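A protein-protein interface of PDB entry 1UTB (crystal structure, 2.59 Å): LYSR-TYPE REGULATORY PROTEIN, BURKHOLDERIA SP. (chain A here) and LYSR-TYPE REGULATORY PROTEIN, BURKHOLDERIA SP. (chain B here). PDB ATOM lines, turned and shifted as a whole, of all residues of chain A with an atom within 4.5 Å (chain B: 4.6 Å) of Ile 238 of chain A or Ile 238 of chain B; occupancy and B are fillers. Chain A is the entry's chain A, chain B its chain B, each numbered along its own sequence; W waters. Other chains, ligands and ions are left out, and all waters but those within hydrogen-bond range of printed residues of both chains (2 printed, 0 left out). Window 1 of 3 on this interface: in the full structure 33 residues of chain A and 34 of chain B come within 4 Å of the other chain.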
ATOM      1  N   ASP A 113      30.955  -8.018 -13.596  1.00  0.00           N
ATOM      2  CA  ASP A 113      30.912  -7.485 -14.942  1.00  0.00           C
ATOM      3  C   ASP A 113      31.016  -5.953 -14.967  1.00  0.00           C
ATOM      4  O   ASP A 113      31.677  -5.405 -15.842  1.00  0.00           O
ATOM      5  CB  ASP A 113      29.685  -8.009 -15.712  1.00  0.00           C
ATOM      6  CG  ASP A 113      28.346  -7.782 -14.981  1.00  0.00           C
ATOM      7  OD1 ASP A 113      27.284  -8.167 -15.549  1.00  0.00           O
ATOM      8  OD2 ASP A 113      28.250  -7.244 -13.848  1.00  0.00           O
ATOM      9  N   GLU A 116      34.635  -5.222 -14.287  1.00  0.00           N
ATOM     10  CA  GLU A 116      35.494  -5.516 -15.422  1.00  0.00           C
ATOM     11  C   GLU A 116      35.444  -4.409 -16.446  1.00  0.00           C
ATOM     12  O   GLU A 116      36.458  -3.977 -16.965  1.00  0.00           O
ATOM     13  CB  GLU A 116      35.042  -6.816 -16.055  1.00  0.00           C
ATOM     14  CG  GLU A 116      36.064  -7.566 -16.886  1.00  0.00           C
ATOM     15  CD  GLU A 116      35.623  -9.012 -17.033  1.00  0.00           C
ATOM     16  OE1 GLU A 116      34.897  -9.319 -18.019  1.00  0.00           O
ATOM     17  OE2 GLU A 116      35.934  -9.822 -16.114  1.00  0.00           O
ATOM     18  N   MET A 117      34.240  -3.962 -16.739  1.00  0.00           N
ATOM     19  CA  MET A 117      34.015  -2.856 -17.656  1.00  0.00           C
ATOM     20  C   MET A 117      34.605  -1.532 -17.155  1.00  0.00           C
ATOM     21  O   MET A 117      35.108  -0.736 -17.918  1.00  0.00           O
ATOM     22  CB  MET A 117      32.528  -2.701 -17.819  1.00  0.00           C
ATOM     23  CG  MET A 117      32.129  -1.989 -19.056  1.00  0.00           C
ATOM     24  SD  MET A 117      30.335  -1.893 -19.034  1.00  0.00           S
ATOM     25  CE  MET A 117      30.086  -1.302 -20.808  1.00  0.00           C
ATOM     26  N   ARG A 140      34.909 -13.972 -12.116  1.00  0.00           N
ATOM     27  CA  ARG A 140      33.829 -13.458 -11.296  1.00  0.00           C
ATOM     28  C   ARG A 140      33.988 -14.001  -9.890  1.00  0.00           C
ATOM     29  O   ARG A 140      34.487 -15.103  -9.728  1.00  0.00           O
ATOM     30  CB  ARG A 140      32.471 -13.857 -11.882  1.00  0.00           C
ATOM     31  CG  ARG A 140      32.175 -13.258 -13.249  1.00  0.00           C
ATOM     32  CD  ARG A 140      31.720 -11.795 -13.235  1.00  0.00           C
ATOM     33  NE  ARG A 140      31.746 -11.235 -14.588  1.00  0.00           N
ATOM     34  CZ  ARG A 140      32.837 -10.819 -15.213  1.00  0.00           C
ATOM     35  NH1 ARG A 140      34.000 -10.822 -14.585  1.00  0.00           N
ATOM     36  NH2 ARG A 140      32.763 -10.376 -16.467  1.00  0.00           N
ATOM     37  N   HIS A 236      22.233 -10.065 -16.440  1.00  0.00           N
ATOM     38  CA  HIS A 236      23.473  -9.291 -16.352  1.00  0.00           C
ATOM     39  C   HIS A 236      23.420  -7.985 -17.168  1.00  0.00           C
ATOM     40  O   HIS A 236      22.419  -7.696 -17.800  1.00  0.00           O
ATOM     41  CB  HIS A 236      24.651 -10.150 -16.825  1.00  0.00           C
ATOM     42  CG  HIS A 236      24.694 -11.514 -16.214  1.00  0.00           C
ATOM     43  ND1 HIS A 236      25.187 -11.748 -14.949  1.00  0.00           N
ATOM     44  CD2 HIS A 236      24.309 -12.719 -16.696  1.00  0.00           C
ATOM     45  CE1 HIS A 236      25.096 -13.038 -14.676  1.00  0.00           C
ATOM     46  NE2 HIS A 236      24.563 -13.650 -15.718  1.00  0.00           N
ATOM     47  N   PHE A 237      24.517  -7.225 -17.176  1.00  0.00           N
ATOM     48  CA  PHE A 237      24.514  -5.837 -17.652  1.00  0.00           C
ATOM     49  C   PHE A 237      24.924  -5.627 -19.092  1.00  0.00           C
ATOM     50  O   PHE A 237      24.821  -4.494 -19.602  1.00  0.00           O
ATOM     51  CB  PHE A 237      25.420  -4.977 -16.762  1.00  0.00           C
ATOM     52  CG  PHE A 237      24.835  -4.691 -15.398  1.00  0.00           C
ATOM     53  CD1 PHE A 237      25.127  -5.493 -14.324  1.00  0.00           C
ATOM     54  CD2 PHE A 237      23.986  -3.621 -15.204  1.00  0.00           C
ATOM     55  CE1 PHE A 237      24.583  -5.226 -13.068  1.00  0.00           C
ATOM     56  CE2 PHE A 237      23.456  -3.361 -13.970  1.00  0.00           C
ATOM     57  CZ  PHE A 237      23.753  -4.173 -12.900  1.00  0.00           C
ATOM     58  N   ILE A 238      25.385  -6.684 -19.757  1.00  0.00           N
ATOM     59  CA  ILE A 238      26.029  -6.534 -21.070  1.00  0.00           C
ATOM     60  C   ILE A 238      25.152  -5.810 -22.080  1.00  0.00           C
ATOM     61  O   ILE A 238      25.637  -4.959 -22.846  1.00  0.00           O
ATOM     62  CB  ILE A 238      26.448  -7.905 -21.672  1.00  0.00           C
ATOM     63  CG1 ILE A 238      27.085  -7.708 -23.040  1.00  0.00           C
ATOM     64  CG2 ILE A 238      25.257  -8.845 -21.841  1.00  0.00           C
ATOM     65  CD1 ILE A 238      27.932  -8.861 -23.478  1.00  0.00           C
ATOM     66  N   ALA A 239      23.864  -6.159 -22.083  1.00  0.00           N
ATOM     67  CA  ALA A 239      22.983  -5.764 -23.172  1.00  0.00           C
ATOM     68  C   ALA A 239      22.233  -4.465 -22.898  1.00  0.00           C
ATOM     69  O   ALA A 239      21.531  -3.988 -23.765  1.00  0.00           O
ATOM     70  CB  ALA A 239      21.997  -6.894 -23.494  1.00  0.00           C
ATOM     71  N   ILE A 240      22.416  -3.876 -21.729  1.00  0.00           N
ATOM     72  CA  ILE A 240      21.680  -2.679 -21.328  1.00  0.00           C
ATOM     73  C   ILE A 240      21.965  -1.457 -22.210  1.00  0.00           C
ATOM     74  O   ILE A 240      21.046  -0.814 -22.698  1.00  0.00           O
ATOM     75  CB  ILE A 240      21.993  -2.350 -19.867  1.00  0.00           C
ATOM     76  CG1 ILE A 240      21.524  -3.483 -18.957  1.00  0.00           C
ATOM     77  CG2 ILE A 240      21.360  -1.041 -19.470  1.00  0.00           C
ATOM     78  CD1 ILE A 240      20.043  -3.732 -18.975  1.00  0.00           C
ATOM     79  N   PRO A 242      23.013  -1.161 -25.443  1.00  0.00           N
ATOM     80  CA  PRO A 242      22.291  -1.312 -26.711  1.00  0.00           C
ATOM     81  C   PRO A 242      20.790  -1.384 -26.567  1.00  0.00           C
ATOM     82  O   PRO A 242      20.103  -0.856 -27.426  1.00  0.00           O
ATOM     83  CB  PRO A 242      22.822  -2.633 -27.257  1.00  0.00           C
ATOM     84  CG  PRO A 242      24.120  -2.773 -26.638  1.00  0.00           C
ATOM     85  CD  PRO A 242      23.999  -2.237 -25.257  1.00  0.00           C
ATOM     86  N   ASP B 113      25.388 -14.295 -23.276  1.00  0.00           N
ATOM     87  CA  ASP B 113      25.600 -12.857 -23.208  1.00  0.00           C
ATOM     88  C   ASP B 113      25.674 -12.244 -24.611  1.00  0.00           C
ATOM     89  O   ASP B 113      25.035 -11.244 -24.857  1.00  0.00           O
ATOM     90  CB  ASP B 113      26.800 -12.492 -22.310  1.00  0.00           C
ATOM     91  CG  ASP B 113      28.136 -13.044 -22.823  1.00  0.00           C
ATOM     92  OD1 ASP B 113      29.200 -12.560 -22.349  1.00  0.00           O
ATOM     93  OD2 ASP B 113      28.233 -13.958 -23.692  1.00  0.00           O
ATOM     94  N   GLU B 116      22.162 -12.148 -25.842  1.00  0.00           N
ATOM     95  CA  GLU B 116      21.391 -11.078 -25.232  1.00  0.00           C
ATOM     96  C   GLU B 116      21.665  -9.746 -25.900  1.00  0.00           C
ATOM     97  O   GLU B 116      20.761  -8.994 -26.221  1.00  0.00           O
ATOM     98  CB  GLU B 116      21.740 -10.979 -23.764  1.00  0.00           C
ATOM     99  CG  GLU B 116      20.689 -10.346 -22.895  1.00  0.00           C
ATOM    100  CD  GLU B 116      20.760 -10.953 -21.525  1.00  0.00           C
ATOM    101  OE1 GLU B 116      21.454 -10.379 -20.635  1.00  0.00           O
ATOM    102  OE2 GLU B 116      20.167 -12.044 -21.371  1.00  0.00           O
ATOM    103  N   MET B 117      22.925  -9.470 -26.149  1.00  0.00           N
ATOM    104  CA  MET B 117      23.282  -8.186 -26.715  1.00  0.00           C
ATOM    105  C   MET B 117      22.882  -8.073 -28.187  1.00  0.00           C
ATOM    106  O   MET B 117      22.578  -6.993 -28.673  1.00  0.00           O
ATOM    107  CB  MET B 117      24.768  -7.928 -26.530  1.00  0.00           C
ATOM    108  CG  MET B 117      25.510  -7.710 -27.826  1.00  0.00           C
ATOM    109  SD  MET B 117      27.107  -7.119 -27.495  1.00  0.00           S
ATOM    110  CE  MET B 117      26.860  -5.875 -26.202  1.00  0.00           C
ATOM    111  N   ARG B 140      20.561 -17.376 -18.743  1.00  0.00           N
ATOM    112  CA  ARG B 140      21.655 -18.098 -19.376  1.00  0.00           C
ATOM    113  C   ARG B 140      21.298 -19.578 -19.400  1.00  0.00           C
ATOM    114  O   ARG B 140      20.618 -20.037 -18.495  1.00  0.00           O
ATOM    115  CB  ARG B 140      22.941 -17.861 -18.590  1.00  0.00           C
ATOM    116  CG  ARG B 140      23.395 -16.432 -18.600  1.00  0.00           C
ATOM    117  CD  ARG B 140      24.096 -16.065 -19.880  1.00  0.00           C
ATOM    118  NE  ARG B 140      24.364 -14.635 -19.978  1.00  0.00           N
ATOM    119  CZ  ARG B 140      23.456 -13.709 -20.275  1.00  0.00           C
ATOM    120  NH1 ARG B 140      22.193 -14.033 -20.513  1.00  0.00           N
ATOM    121  NH2 ARG B 140      23.827 -12.440 -20.336  1.00  0.00           N
ATOM    122  N   HIS B 236      34.121 -13.196 -20.000  1.00  0.00           N
ATOM    123  CA  HIS B 236      32.891 -12.846 -20.735  1.00  0.00           C
ATOM    124  C   HIS B 236      33.104 -11.617 -21.590  1.00  0.00           C
ATOM    125  O   HIS B 236      34.138 -10.965 -21.489  1.00  0.00           O
ATOM    126  CB  HIS B 236      31.766 -12.583 -19.763  1.00  0.00           C
ATOM    127  CG  HIS B 236      31.444 -13.740 -18.871  1.00  0.00           C
ATOM    128  ND1 HIS B 236      30.846 -14.894 -19.334  1.00  0.00           N
ATOM    129  CD2 HIS B 236      31.606 -13.909 -17.537  1.00  0.00           C
ATOM    130  CE1 HIS B 236      30.670 -15.729 -18.324  1.00  0.00           C
ATOM    131  NE2 HIS B 236      31.109 -15.151 -17.220  1.00  0.00           N
ATOM    132  N   PHE B 237      32.126 -11.300 -22.426  1.00  0.00           N
ATOM    133  CA  PHE B 237      32.312 -10.268 -23.453  1.00  0.00           C
ATOM    134  C   PHE B 237      32.049  -8.792 -23.049  1.00  0.00           C
ATOM    135  O   PHE B 237      32.399  -7.890 -23.791  1.00  0.00           O
ATOM    136  CB  PHE B 237      31.480 -10.616 -24.694  1.00  0.00           C
ATOM    137  CG  PHE B 237      32.027 -11.766 -25.479  1.00  0.00           C
ATOM    138  CD1 PHE B 237      31.575 -13.068 -25.238  1.00  0.00           C
ATOM    139  CD2 PHE B 237      32.989 -11.558 -26.463  1.00  0.00           C
ATOM    140  CE1 PHE B 237      32.073 -14.147 -25.969  1.00  0.00           C
ATOM    141  CE2 PHE B 237      33.497 -12.647 -27.202  1.00  0.00           C
ATOM    142  CZ  PHE B 237      33.031 -13.938 -26.943  1.00  0.00           C
ATOM    143  N   ILE B 238      31.482  -8.557 -21.878  1.00  0.00           N
ATOM    144  CA  ILE B 238      30.999  -7.223 -21.519  1.00  0.00           C
ATOM    145  C   ILE B 238      31.978  -6.082 -21.713  1.00  0.00           C
ATOM    146  O   ILE B 238      31.595  -5.037 -22.219  1.00  0.00           O
ATOM    147  CB  ILE B 238      30.453  -7.182 -20.086  1.00  0.00           C
ATOM    148  CG1 ILE B 238      29.866  -5.804 -19.802  1.00  0.00           C
ATOM    149  CG2 ILE B 238      31.532  -7.529 -19.071  1.00  0.00           C
ATOM    150  CD1 ILE B 238      29.024  -5.760 -18.592  1.00  0.00           C
ATOM    151  N   ALA B 239      33.234  -6.280 -21.334  1.00  0.00           N
ATOM    152  CA  ALA B 239      34.219  -5.195 -21.317  1.00  0.00           C
ATOM    153  C   ALA B 239      35.085  -5.128 -22.562  1.00  0.00           C
ATOM    154  O   ALA B 239      36.017  -4.319 -22.617  1.00  0.00           O
ATOM    155  CB  ALA B 239      35.100  -5.330 -20.101  1.00  0.00           C
ATOM    156  N   ILE B 240      34.789  -5.931 -23.579  1.00  0.00           N
ATOM    157  CA  ILE B 240      35.671  -5.990 -24.739  1.00  0.00           C
ATOM    158  C   ILE B 240      35.719  -4.672 -25.481  1.00  0.00           C
ATOM    159  O   ILE B 240      36.797  -4.210 -25.835  1.00  0.00           O
ATOM    160  CB  ILE B 240      35.288  -7.142 -25.701  1.00  0.00           C
ATOM    161  CG1 ILE B 240      35.471  -8.489 -25.008  1.00  0.00           C
ATOM    162  CG2 ILE B 240      36.159  -7.100 -26.971  1.00  0.00           C
ATOM    163  CD1 ILE B 240      36.934  -8.827 -24.676  1.00  0.00           C
ATOM    164  N   PRO B 242      34.979  -1.372 -24.552  1.00  0.00           N
ATOM    165  CA  PRO B 242      35.763  -0.405 -23.774  1.00  0.00           C
ATOM    166  C   PRO B 242      37.254  -0.722 -23.720  1.00  0.00           C
ATOM    167  O   PRO B 242      38.064   0.198 -23.882  1.00  0.00           O
ATOM    168  CB  PRO B 242      35.184  -0.523 -22.380  1.00  0.00           C
ATOM    169  CG  PRO B 242      33.850  -1.135 -22.540  1.00  0.00           C
ATOM    170  CD  PRO B 242      33.821  -1.883 -23.806  1.00  0.00           C
HETATM  171  O   HOH W   1      22.118  -7.937 -20.427  1.00  0.00           O
HETATM  172  O   HOH W   2      34.667  -8.569 -20.354  1.00  0.00           O
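The side-chain carboxylate (OD1) of Asp 113 of chain A lies within hydrogen-bond range of the backbone NH (N) of Phe 237 of chain A (3.3 Å).
The guanidinium group (NH1) of Arg 140 of chain A lies within salt-bridge range of the side-chain carboxylate (OE2) of Glu 116 of chain A (2.7 Å).
The side-chain carboxylate (OD1) of Asp 113 of chain B sits at hydrogen-bond distance from the backbone NH (N) of Phe 237 of chain B (3.2 Å).
The side-chain carboxylate of Glu 116 of chain B lies within salt-bridge range of the guanidinium group of Arg 140 of chain B (3.0 Å).
Printed residues of chain A that touch a printed residue of chain B: Asp 113, Glu 116, Met 117, Arg 140, His 236, Ile 238 and Ala 239.
Hydrophobic or aromatic side chains of chain A that line the printed part of chain B: Met 117, His 236, Ile 238 and Ala 239.
Among the printed residues, 13 pairs touch across the chains.
Among the printed residues, no Asp or Glu carboxylate lies within 4 Å of a Lys or Arg side-chain nitrogen of the other chain.
Water W2 lies within hydrogen-bond range of the side-chain carboxylate (OE1) of Glu 116 of chain A (2.5 Å), the backbone carbonyl oxygen (O) of His 236 of chain B (2.7 Å) and the backbone NH (N) of Ala 239 of chain B (2.9 Å).
Water W1 lies within hydrogen-bond range of the side-chain carboxylate of Glu 116 of chain B (2.5 Å), the backbone carbonyl oxygen of His 236 of chain A (2.7 Å) and the backbone NH of Ala 239 of chain A (3.0 Å).
Among the printed residues, pairs that only touch across the chains: Asp 113 of chain A with Ile 238 of chain B, Glu 116 of chain A with His 236 of chain B, Glu 116 of chain A with Ile 238 of chain B, Glu 116 of chain A with Ala 239 of chain B, Met 117 of chain A with Ala 239 of chain B, Met 117 of chain A with Pro 242 of chain B, Arg 140 of chain A with His 236 of chain B, His 236 of chain A with Arg 140 of chain B, Ile 238 of chain A with Asp 113 of chain B, Ile 238 of chain A with Met 117 of chain B, Ile 238 of chain A with Ile 238 of chain B, Ala 239 of chain A with Glu 116 of chain B and Ala 239 of chain A with Met 117 of chain B.
Of the printed residues of chain B, Asp 113 of chain A touches Ile 238 (3.7 Å).
Of the printed residues of chain B, Met 117 of chain A touches Ala 239 (3.6 Å) and Pro 242 (3.98 Å).
Of the printed residues of chain B, His 236 of chain A touches Arg 140.
Printed residues of chain A within 4 Å of Asp 113 of chain B: Ile 238 (3.9 Å).
Of the printed residues of chain A, Glu 116 of chain B touches Ala 239 (3.7 Å).
Printed residues of chain A within 4 Å of Ile 238 of chain B: Asp 113, Glu 116 and Ile 238.
The nearest printed residue of chain B that does not touch Ile 238 of chain A is Phe 237 of chain B (4.1 Å).
The nearest printed residue of chain B that does not touch Asp 113 of chain A is Ala 239 of chain B (5.5 Å).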
